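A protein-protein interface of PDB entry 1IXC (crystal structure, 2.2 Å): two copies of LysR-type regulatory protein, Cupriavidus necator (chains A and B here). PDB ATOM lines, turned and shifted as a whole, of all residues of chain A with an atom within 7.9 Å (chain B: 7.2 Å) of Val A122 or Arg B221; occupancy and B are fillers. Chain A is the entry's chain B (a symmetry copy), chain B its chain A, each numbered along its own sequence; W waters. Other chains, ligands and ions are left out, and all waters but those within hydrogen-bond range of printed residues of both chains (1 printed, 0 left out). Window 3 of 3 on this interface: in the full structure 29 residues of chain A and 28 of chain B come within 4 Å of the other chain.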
ATOM      1  N   GLY A  91      -1.981  26.566   9.777  1.00  0.00           N
ATOM      2  CA  GLY A  91      -0.637  26.282   9.316  1.00  0.00           C
ATOM      3  C   GLY A  91      -0.431  24.779   9.180  1.00  0.00           C
ATOM      4  O   GLY A  91      -1.231  23.983   9.680  1.00  0.00           O
ATOM      5  N   GLU A  92       0.617  24.399   8.460  1.00  0.00           N
ATOM      6  CA  GLU A  92       1.001  23.005   8.350  1.00  0.00           C
ATOM      7  C   GLU A  92       2.306  22.727   9.106  1.00  0.00           C
ATOM      8  O   GLU A  92       3.361  23.201   8.709  1.00  0.00           O
ATOM      9  CB  GLU A  92       1.182  22.594   6.895  1.00  0.00           C
ATOM     10  CG  GLU A  92       1.803  21.211   6.765  1.00  0.00           C
ATOM     11  CD  GLU A  92       2.049  20.817   5.325  1.00  0.00           C
ATOM     12  OE1 GLU A  92       3.182  21.034   4.842  1.00  0.00           O
ATOM     13  OE2 GLU A  92       1.114  20.294   4.685  1.00  0.00           O
ATOM     14  N   LEU A  93       2.206  21.964  10.191  1.00  0.00           N
ATOM     15  CA  LEU A  93       3.364  21.509  10.952  1.00  0.00           C
ATOM     16  C   LEU A  93       4.068  20.385  10.192  1.00  0.00           C
ATOM     17  O   LEU A  93       3.496  19.313   9.965  1.00  0.00           O
ATOM     18  CB  LEU A  93       2.918  20.988  12.314  1.00  0.00           C
ATOM     19  CG  LEU A  93       4.022  20.511  13.254  1.00  0.00           C
ATOM     20  CD1 LEU A  93       4.775  21.695  13.819  1.00  0.00           C
ATOM     21  CD2 LEU A  93       3.438  19.652  14.377  1.00  0.00           C
ATOM     22  N   SER A  94       5.297  20.649   9.772  1.00  0.00           N
ATOM     23  CA  SER A  94       6.146  19.662   9.110  1.00  0.00           C
ATOM     24  C   SER A  94       6.928  18.882  10.172  1.00  0.00           C
ATOM     25  O   SER A  94       7.788  19.448  10.890  1.00  0.00           O
ATOM     26  CB  SER A  94       7.099  20.376   8.153  1.00  0.00           C
ATOM     27  OG  SER A  94       7.898  19.450   7.443  1.00  0.00           O
ATOM     28  N   VAL A  95       6.604  17.590  10.267  1.00  0.00           N
ATOM     29  CA  VAL A  95       7.139  16.670  11.259  1.00  0.00           C
ATOM     30  C   VAL A  95       7.991  15.620  10.583  1.00  0.00           C
ATOM     31  O   VAL A  95       7.628  15.094   9.534  1.00  0.00           O
ATOM     32  CB  VAL A  95       5.993  15.929  12.019  1.00  0.00           C
ATOM     33  CG1 VAL A  95       6.550  14.921  13.005  1.00  0.00           C
ATOM     34  CG2 VAL A  95       5.083  16.921  12.745  1.00  0.00           C
ATOM     35  N   LEU A 110       0.139  13.816  18.165  1.00  0.00           N
ATOM     36  CA  LEU A 110      -0.457  14.574  17.072  1.00  0.00           C
ATOM     37  C   LEU A 110      -1.980  14.673  17.215  1.00  0.00           C
ATOM     38  O   LEU A 110      -2.571  15.684  16.847  1.00  0.00           O
ATOM     39  CB  LEU A 110      -0.104  13.945  15.724  1.00  0.00           C
ATOM     40  CG  LEU A 110       1.399  13.903  15.420  1.00  0.00           C
ATOM     41  CD1 LEU A 110       1.652  13.118  14.159  1.00  0.00           C
ATOM     42  CD2 LEU A 110       1.990  15.314  15.292  1.00  0.00           C
ATOM     43  N   ARG A 111      -2.619  13.613  17.709  1.00  0.00           N
ATOM     44  CA  ARG A 111      -4.062  13.632  17.970  1.00  0.00           C
ATOM     45  C   ARG A 111      -4.385  14.773  18.945  1.00  0.00           C
ATOM     46  O   ARG A 111      -5.259  15.603  18.695  1.00  0.00           O
ATOM     47  CB  ARG A 111      -4.497  12.274  18.542  1.00  0.00           C
ATOM     48  CG  ARG A 111      -5.926  12.153  19.094  1.00  0.00           C
ATOM     49  CD  ARG A 111      -7.022  12.157  18.051  1.00  0.00           C
ATOM     50  NE  ARG A 111      -8.343  11.943  18.656  1.00  0.00           N
ATOM     51  CZ  ARG A 111      -9.512  12.184  18.056  1.00  0.00           C
ATOM     52  NH1 ARG A 111      -9.562  12.652  16.805  1.00  0.00           N
ATOM     53  NH2 ARG A 111     -10.643  11.947  18.711  1.00  0.00           N
ATOM     54  N   PHE A 113      -2.723  17.393  19.634  1.00  0.00           N
ATOM     55  CA  PHE A 113      -2.398  18.708  19.088  1.00  0.00           C
ATOM     56  C   PHE A 113      -3.460  19.178  18.119  1.00  0.00           C
ATOM     57  O   PHE A 113      -3.920  20.313  18.188  1.00  0.00           O
ATOM     58  CB  PHE A 113      -1.052  18.674  18.368  1.00  0.00           C
ATOM     59  CG  PHE A 113      -0.791  19.883  17.503  1.00  0.00           C
ATOM     60  CD1 PHE A 113      -0.471  21.092  18.071  1.00  0.00           C
ATOM     61  CD2 PHE A 113      -0.854  19.794  16.121  1.00  0.00           C
ATOM     62  CE1 PHE A 113      -0.225  22.194  17.285  1.00  0.00           C
ATOM     63  CE2 PHE A 113      -0.613  20.897  15.327  1.00  0.00           C
ATOM     64  CZ  PHE A 113      -0.294  22.097  15.909  1.00  0.00           C
ATOM     65  N   LEU A 114      -3.808  18.305  17.182  1.00  0.00           N
ATOM     66  CA  LEU A 114      -4.831  18.601  16.197  1.00  0.00           C
ATOM     67  C   LEU A 114      -6.177  18.859  16.883  1.00  0.00           C
ATOM     68  O   LEU A 114      -7.006  19.605  16.365  1.00  0.00           O
ATOM     69  CB  LEU A 114      -4.964  17.436  15.205  1.00  0.00           C
ATOM     70  CG  LEU A 114      -3.828  17.297  14.180  1.00  0.00           C
ATOM     71  CD1 LEU A 114      -3.893  15.972  13.495  1.00  0.00           C
ATOM     72  CD2 LEU A 114      -3.856  18.413  13.136  1.00  0.00           C
ATOM     73  N   THR A 119      -7.901  23.374  12.984  1.00  0.00           N
ATOM     74  CA  THR A 119      -7.741  23.902  11.625  1.00  0.00           C
ATOM     75  C   THR A 119      -6.287  23.857  11.166  1.00  0.00           C
ATOM     76  O   THR A 119      -5.934  24.433  10.137  1.00  0.00           O
ATOM     77  CB  THR A 119      -8.273  25.334  11.523  1.00  0.00           C
ATOM     78  OG1 THR A 119      -7.715  26.143  12.569  1.00  0.00           O
ATOM     79  CG2 THR A 119      -9.773  25.366  11.775  1.00  0.00           C
ATOM     80  N   ALA A 120      -5.435  23.209  11.954  1.00  0.00           N
ATOM     81  CA  ALA A 120      -4.051  22.985  11.562  1.00  0.00           C
ATOM     82  C   ALA A 120      -3.958  21.675  10.792  1.00  0.00           C
ATOM     83  O   ALA A 120      -4.866  20.845  10.867  1.00  0.00           O
ATOM     84  CB  ALA A 120      -3.174  22.914  12.791  1.00  0.00           C
ATOM     85  N   THR A 121      -2.890  21.514  10.019  1.00  0.00           N
ATOM     86  CA  THR A 121      -2.584  20.226   9.400  1.00  0.00           C
ATOM     87  C   THR A 121      -1.157  19.811   9.709  1.00  0.00           C
ATOM     88  O   THR A 121      -0.371  20.589  10.235  1.00  0.00           O
ATOM     89  CB  THR A 121      -2.789  20.222   7.863  1.00  0.00           C
ATOM     90  OG1 THR A 121      -1.747  20.969   7.218  1.00  0.00           O
ATOM     91  CG2 THR A 121      -4.078  20.901   7.467  1.00  0.00           C
ATOM     92  N   VAL A 122      -0.846  18.558   9.389  1.00  0.00           N
ATOM     93  CA  VAL A 122       0.491  18.024   9.554  1.00  0.00           C
ATOM     94  C   VAL A 122       0.947  17.270   8.312  1.00  0.00           C
ATOM     95  O   VAL A 122       0.137  16.742   7.570  1.00  0.00           O
ATOM     96  CB  VAL A 122       0.572  17.069  10.758  1.00  0.00           C
ATOM     97  CG1 VAL A 122       0.254  17.796  12.048  1.00  0.00           C
ATOM     98  CG2 VAL A 122      -0.353  15.903  10.602  1.00  0.00           C
ATOM     99  N   SER A 123       2.248  17.272   8.070  1.00  0.00           N
ATOM    100  CA  SER A 123       2.848  16.381   7.099  1.00  0.00           C
ATOM    101  C   SER A 123       3.856  15.552   7.865  1.00  0.00           C
ATOM    102  O   SER A 123       4.342  15.990   8.928  1.00  0.00           O
ATOM    103  CB  SER A 123       3.547  17.149   5.996  1.00  0.00           C
ATOM    104  OG  SER A 123       4.557  17.938   6.575  1.00  0.00           O
ATOM    105  N   LEU A 124       4.178  14.377   7.330  1.00  0.00           N
ATOM    106  CA  LEU A 124       5.118  13.451   7.965  1.00  0.00           C
ATOM    107  C   LEU A 124       6.165  12.995   6.975  1.00  0.00           C
ATOM    108  O   LEU A 124       5.847  12.668   5.835  1.00  0.00           O
ATOM    109  CB  LEU A 124       4.401  12.194   8.465  1.00  0.00           C
ATOM    110  CG  LEU A 124       3.608  12.304   9.752  1.00  0.00           C
ATOM    111  CD1 LEU A 124       2.736  11.073   9.915  1.00  0.00           C
ATOM    112  CD2 LEU A 124       4.546  12.457  10.943  1.00  0.00           C
ATOM    113  N   THR A 125       7.417  12.973   7.404  1.00  0.00           N
ATOM    114  CA  THR A 125       8.485  12.435   6.576  1.00  0.00           C
ATOM    115  C   THR A 125       9.455  11.610   7.411  1.00  0.00           C
ATOM    116  O   THR A 125       9.949  12.081   8.439  1.00  0.00           O
ATOM    117  CB  THR A 125       9.298  13.563   5.943  1.00  0.00           C
ATOM    118  OG1 THR A 125       8.442  14.601   5.455  1.00  0.00           O
ATOM    119  CG2 THR A 125      10.006  13.073   4.707  1.00  0.00           C
ATOM    120  N   ILE A 280       3.050  27.974  14.201  1.00  0.00           N
ATOM    121  CA  ILE A 280       2.481  26.639  14.250  1.00  0.00           C
ATOM    122  C   ILE A 280       3.380  25.723  15.095  1.00  0.00           C
ATOM    123  O   ILE A 280       2.887  24.873  15.831  1.00  0.00           O
ATOM    124  CB  ILE A 280       2.224  26.055  12.829  1.00  0.00           C
ATOM    125  CG1 ILE A 280       1.504  24.711  12.948  1.00  0.00           C
ATOM    126  CG2 ILE A 280       3.516  25.891  12.025  1.00  0.00           C
ATOM    127  CD1 ILE A 280       0.086  24.809  13.516  1.00  0.00           C
ATOM    128  N   PHE A 284       2.931  23.910  18.815  1.00  0.00           N
ATOM    129  CA  PHE A 284       3.150  22.472  18.977  1.00  0.00           C
ATOM    130  C   PHE A 284       4.087  22.205  20.141  1.00  0.00           C
ATOM    131  O   PHE A 284       3.844  21.305  20.925  1.00  0.00           O
ATOM    132  CB  PHE A 284       3.726  21.837  17.705  1.00  0.00           C
ATOM    133  CG  PHE A 284       3.933  20.348  17.813  1.00  0.00           C
ATOM    134  CD1 PHE A 284       2.855  19.489  17.814  1.00  0.00           C
ATOM    135  CD2 PHE A 284       5.208  19.812  17.929  1.00  0.00           C
ATOM    136  CE1 PHE A 284       3.038  18.114  17.910  1.00  0.00           C
ATOM    137  CE2 PHE A 284       5.401  18.432  18.026  1.00  0.00           C
ATOM    138  CZ  PHE A 284       4.307  17.584  18.012  1.00  0.00           C
ATOM    139  N   GLU B 190     -12.605  11.924   2.246  1.00  0.00           N
ATOM    140  CA  GLU B 190     -11.307  12.500   1.880  1.00  0.00           C
ATOM    141  C   GLU B 190     -10.222  11.441   2.134  1.00  0.00           C
ATOM    142  O   GLU B 190      -9.955  11.078   3.265  1.00  0.00           O
ATOM    143  CB  GLU B 190     -11.019  13.758   2.699  1.00  0.00           C
ATOM    144  CG  GLU B 190     -11.973  14.932   2.483  1.00  0.00           C
ATOM    145  CD  GLU B 190     -11.761  15.686   1.172  1.00  0.00           C
ATOM    146  OE1 GLU B 190     -10.598  15.948   0.765  1.00  0.00           O
ATOM    147  OE2 GLU B 190     -12.787  16.042   0.545  1.00  0.00           O
ATOM    148  N   LEU B 191      -9.595  10.957   1.077  1.00  0.00           N
ATOM    149  CA  LEU B 191      -8.677   9.842   1.192  1.00  0.00           C
ATOM    150  C   LEU B 191      -7.209  10.273   1.127  1.00  0.00           C
ATOM    151  O   LEU B 191      -6.829  11.124   0.331  1.00  0.00           O
ATOM    152  CB  LEU B 191      -8.940   8.818   0.086  1.00  0.00           C
ATOM    153  CG  LEU B 191     -10.243   8.011   0.164  1.00  0.00           C
ATOM    154  CD1 LEU B 191     -10.453   7.301  -1.129  1.00  0.00           C
ATOM    155  CD2 LEU B 191     -10.207   6.990   1.308  1.00  0.00           C
ATOM    156  N   THR B 192      -6.418   9.634   1.972  1.00  0.00           N
ATOM    157  CA  THR B 192      -4.991   9.798   2.045  1.00  0.00           C
ATOM    158  C   THR B 192      -4.423   8.507   1.512  1.00  0.00           C
ATOM    159  O   THR B 192      -4.541   7.459   2.145  1.00  0.00           O
ATOM    160  CB  THR B 192      -4.585   9.995   3.500  1.00  0.00           C
ATOM    161  OG1 THR B 192      -5.023  11.286   3.926  1.00  0.00           O
ATOM    162  CG2 THR B 192      -3.050  10.002   3.671  1.00  0.00           C
ATOM    163  N   LEU B 193      -3.843   8.586   0.322  1.00  0.00           N
ATOM    164  CA  LEU B 193      -3.330   7.429  -0.362  1.00  0.00           C
ATOM    165  C   LEU B 193      -1.822   7.461  -0.310  1.00  0.00           C
ATOM    166  O   LEU B 193      -1.232   8.402   0.208  1.00  0.00           O
ATOM    167  CB  LEU B 193      -3.822   7.425  -1.811  1.00  0.00           C
ATOM    168  CG  LEU B 193      -5.339   7.338  -1.995  1.00  0.00           C
ATOM    169  CD1 LEU B 193      -5.631   6.917  -3.377  1.00  0.00           C
ATOM    170  CD2 LEU B 193      -5.980   6.377  -1.064  1.00  0.00           C
ATOM    171  N   PHE B 194      -1.206   6.426  -0.856  1.00  0.00           N
ATOM    172  CA  PHE B 194       0.231   6.279  -0.827  1.00  0.00           C
ATOM    173  C   PHE B 194       0.603   5.198  -1.823  1.00  0.00           C
ATOM    174  O   PHE B 194      -0.261   4.458  -2.254  1.00  0.00           O
ATOM    175  CB  PHE B 194       0.644   5.803   0.567  1.00  0.00           C
ATOM    176  CG  PHE B 194      -0.060   4.540   0.993  1.00  0.00           C
ATOM    177  CD1 PHE B 194       0.460   3.312   0.688  1.00  0.00           C
ATOM    178  CD2 PHE B 194      -1.263   4.600   1.672  1.00  0.00           C
ATOM    179  CE1 PHE B 194      -0.201   2.152   1.047  1.00  0.00           C
ATOM    180  CE2 PHE B 194      -1.928   3.445   2.037  1.00  0.00           C
ATOM    181  CZ  PHE B 194      -1.400   2.227   1.731  1.00  0.00           C
ATOM    182  N   ARG B 218     -12.200  11.248  -3.918  1.00  0.00           N
ATOM    183  CA  ARG B 218     -11.744  12.478  -3.275  1.00  0.00           C
ATOM    184  C   ARG B 218     -10.382  12.215  -2.640  1.00  0.00           C
ATOM    185  O   ARG B 218     -10.277  11.457  -1.675  1.00  0.00           O
ATOM    186  CB  ARG B 218     -12.687  12.868  -2.154  1.00  0.00           C
ATOM    187  CG  ARG B 218     -13.937  13.565  -2.552  1.00  0.00           C
ATOM    188  CD  ARG B 218     -14.612  14.188  -1.348  1.00  0.00           C
ATOM    189  NE  ARG B 218     -15.420  15.355  -1.662  1.00  0.00           N
ATOM    190  CZ  ARG B 218     -16.576  15.323  -2.308  1.00  0.00           C
ATOM    191  NH1 ARG B 218     -17.072  14.181  -2.773  1.00  0.00           N
ATOM    192  NH2 ARG B 218     -17.233  16.450  -2.515  1.00  0.00           N
ATOM    193  N   ILE B 219      -9.347  12.845  -3.172  1.00  0.00           N
ATOM    194  CA  ILE B 219      -7.994  12.650  -2.695  1.00  0.00           C
ATOM    195  C   ILE B 219      -7.522  13.896  -1.952  1.00  0.00           C
ATOM    196  O   ILE B 219      -7.242  14.928  -2.562  1.00  0.00           O
ATOM    197  CB  ILE B 219      -7.035  12.337  -3.867  1.00  0.00           C
ATOM    198  CG1 ILE B 219      -7.587  11.217  -4.755  1.00  0.00           C
ATOM    199  CG2 ILE B 219      -5.607  11.974  -3.339  1.00  0.00           C
ATOM    200  CD1 ILE B 219      -7.915   9.907  -4.011  1.00  0.00           C
ATOM    201  N   ALA B 220      -7.428  13.786  -0.633  1.00  0.00           N
ATOM    202  CA  ALA B 220      -6.910  14.869   0.197  1.00  0.00           C
ATOM    203  C   ALA B 220      -5.421  15.056  -0.016  1.00  0.00           C
ATOM    204  O   ALA B 220      -4.935  16.180  -0.054  1.00  0.00           O
ATOM    205  CB  ALA B 220      -7.170  14.569   1.668  1.00  0.00           C
ATOM    206  N   ARG B 221      -4.703  13.936  -0.089  1.00  0.00           N
ATOM    207  CA  ARG B 221      -3.265  13.945  -0.258  1.00  0.00           C
ATOM    208  C   ARG B 221      -2.705  12.580  -0.615  1.00  0.00           C
ATOM    209  O   ARG B 221      -3.348  11.546  -0.437  1.00  0.00           O
ATOM    210  CB  ARG B 221      -2.609  14.402   1.049  1.00  0.00           C
ATOM    211  CG  ARG B 221      -3.202  13.747   2.295  1.00  0.00           C
ATOM    212  CD  ARG B 221      -2.542  14.178   3.617  1.00  0.00           C
ATOM    213  NE  ARG B 221      -3.467  13.954   4.730  1.00  0.00           N
ATOM    214  CZ  ARG B 221      -3.354  14.511   5.925  1.00  0.00           C
ATOM    215  NH1 ARG B 221      -2.308  15.271   6.211  1.00  0.00           N
ATOM    216  NH2 ARG B 221      -4.277  14.274   6.848  1.00  0.00           N
ATOM    217  N   VAL B 222      -1.491  12.596  -1.136  1.00  0.00           N
ATOM    218  CA  VAL B 222      -0.739  11.370  -1.344  1.00  0.00           C
ATOM    219  C   VAL B 222       0.509  11.479  -0.471  1.00  0.00           C
ATOM    220  O   VAL B 222       1.295  12.411  -0.596  1.00  0.00           O
ATOM    221  CB  VAL B 222      -0.383  11.122  -2.820  1.00  0.00           C
ATOM    222  CG1 VAL B 222       0.168   9.711  -2.988  1.00  0.00           C
ATOM    223  CG2 VAL B 222      -1.626  11.275  -3.686  1.00  0.00           C
ATOM    224  N   VAL B 223       0.660  10.523   0.439  1.00  0.00           N
ATOM    225  CA  VAL B 223       1.752  10.547   1.411  1.00  0.00           C
ATOM    226  C   VAL B 223       2.803   9.535   1.000  1.00  0.00           C
ATOM    227  O   VAL B 223       2.582   8.737   0.077  1.00  0.00           O
ATOM    228  CB  VAL B 223       1.238  10.365   2.852  1.00  0.00           C
ATOM    229  CG1 VAL B 223       0.304  11.492   3.188  1.00  0.00           C
ATOM    230  CG2 VAL B 223       0.549   9.043   3.039  1.00  0.00           C
ATOM    231  N   LEU B 232      -1.286   8.980  10.365  1.00  0.00           N
ATOM    232  CA  LEU B 232      -2.291  10.047  10.215  1.00  0.00           C
ATOM    233  C   LEU B 232      -3.719   9.546  10.562  1.00  0.00           C
ATOM    234  O   LEU B 232      -4.483  10.244  11.222  1.00  0.00           O
ATOM    235  CB  LEU B 232      -2.250  10.635   8.797  1.00  0.00           C
ATOM    236  CG  LEU B 232      -0.980  11.470   8.494  1.00  0.00           C
ATOM    237  CD1 LEU B 232      -0.791  11.737   7.020  1.00  0.00           C
ATOM    238  CD2 LEU B 232      -0.934  12.793   9.274  1.00  0.00           C
ATOM    239  N   THR B 233      -4.078   8.334  10.140  1.00  0.00           N
ATOM    240  CA  THR B 233      -5.403   7.803  10.466  1.00  0.00           C
ATOM    241  C   THR B 233      -5.534   7.556  11.964  1.00  0.00           C
ATOM    242  O   THR B 233      -6.556   7.843  12.593  1.00  0.00           O
ATOM    243  CB  THR B 233      -5.628   6.508   9.727  1.00  0.00           C
ATOM    244  OG1 THR B 233      -5.569   6.751   8.316  1.00  0.00           O
ATOM    245  CG2 THR B 233      -7.021   5.952   9.981  1.00  0.00           C
ATOM    246  N   ALA B 235      -3.896   9.216  14.211  1.00  0.00           N
ATOM    247  CA  ALA B 235      -3.954  10.551  14.860  1.00  0.00           C
ATOM    248  C   ALA B 235      -5.294  11.255  14.679  1.00  0.00           C
ATOM    249  O   ALA B 235      -5.460  12.334  15.193  1.00  0.00           O
ATOM    250  CB  ALA B 235      -2.850  11.414  14.318  1.00  0.00           C
ATOM    251  N   GLY B 236      -6.202  10.684  13.884  1.00  0.00           N
ATOM    252  CA  GLY B 236      -7.550  11.211  13.716  1.00  0.00           C
ATOM    253  C   GLY B 236      -7.605  12.180  12.549  1.00  0.00           C
ATOM    254  O   GLY B 236      -8.602  12.864  12.347  1.00  0.00           O
ATOM    255  N   ALA B 237      -6.533  12.220  11.763  1.00  0.00           N
ATOM    256  CA  ALA B 237      -6.398  13.233  10.709  1.00  0.00           C
ATOM    257  C   ALA B 237      -6.681  12.724   9.319  1.00  0.00           C
ATOM    258  O   ALA B 237      -6.600  13.484   8.386  1.00  0.00           O
ATOM    259  CB  ALA B 237      -4.977  13.778  10.718  1.00  0.00           C
ATOM    260  N   ALA B 238      -6.982  11.446   9.167  1.00  0.00           N
ATOM    261  CA  ALA B 238      -7.104  10.883   7.828  1.00  0.00           C
ATOM    262  C   ALA B 238      -7.982   9.655   7.766  1.00  0.00           C
ATOM    263  O   ALA B 238      -8.310   9.052   8.787  1.00  0.00           O
ATOM    264  CB  ALA B 238      -5.725  10.520   7.310  1.00  0.00           C
ATOM    265  N   SER B 239      -8.379   9.327   6.539  1.00  0.00           N
ATOM    266  CA  SER B 239      -8.911   8.015   6.213  1.00  0.00           C
ATOM    267  C   SER B 239      -8.066   7.511   5.041  1.00  0.00           C
ATOM    268  O   SER B 239      -7.501   8.318   4.287  1.00  0.00           O
ATOM    269  CB  SER B 239     -10.382   8.084   5.825  1.00  0.00           C
ATOM    270  OG  SER B 239     -11.104   8.839   6.778  1.00  0.00           O
HETATM  271  O   HOH W   1      -3.544  16.826   8.826  1.00  0.00           O
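NH1 of Arg B221 sits at hydrogen-bond distance from O of Val A122 (3.2 Å).
The backbone carbonyl oxygen (O) of Leu B232 sits at hydrogen-bond distance from the backbone NH (N) of Ala B238.
OG1 of Thr B192 is in hydrogen-bond range of NE of Arg B221, at 3.2 Å.
The backbone carbonyl oxygen of Leu B232 is in hydrogen-bond range of the backbone NH of Ala B237.
O of Arg B221 is in hydrogen-bond range of N of Leu B193.
O of Ala B237 is in hydrogen-bond range of NH2 of Arg B221, 2.9 Å away.
Among the printed residues, pairs that only touch across the chains: Arg A111 with Ala B235, Val A122 with Leu B232, Leu A114 with Ala B237, Arg A111 with Gly B236, Leu A110 with Ala B235 and Leu A124 with Leu B232.
Ser A94 touches none of the printed residues of chain B.
Val A95 touches none of the printed residues of chain B.
Of the printed residues of chain B, Arg A111 touches Ala B235 (3.3 Å) and Gly B236 (3.96 Å).
Of chain B, only Arg B221 and Leu B232 come within 4 Å of Val A122.
Arg B221 touches one residue of chain A.
Of the printed residues of chain A, Ala B237 touches Leu A114 (3.7 Å).
The nearest printed residue of chain A that does not touch Ala B235 is Leu A114 (4.3 Å).
Of the 18 printed residues of chain A, 5 touch a printed residue of chain B.
Hydrophobic or aromatic side chains of chain A within 4 Å of the printed part of chain B: Leu A110, Leu A114, Val A122 and Leu A124.
Along chain A the printed residues that touch a printed residue of chain B span positions 110 to 124.
Of the 18 printed residues of chain B, 5 touch a printed residue of chain A.
Hydrophobic or aromatic side chains of chain B within 4 Å of the printed part of chain A: Leu B232, Ala B235 and Ala B237.
Among the printed residues, no Asp or Glu carboxylate lies within 4 Å of a Lys or Arg side-chain nitrogen of the other chain.
No position is printed for both chains.
Of the 7 pairs that touch across the chains among the printed residues, none has its exchanged pair printed and touching as well.
Water W1 bridges the backbone NH of Val A122 (3.3 Å) and the guanidinium group of Arg B221 (3.3 Å).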
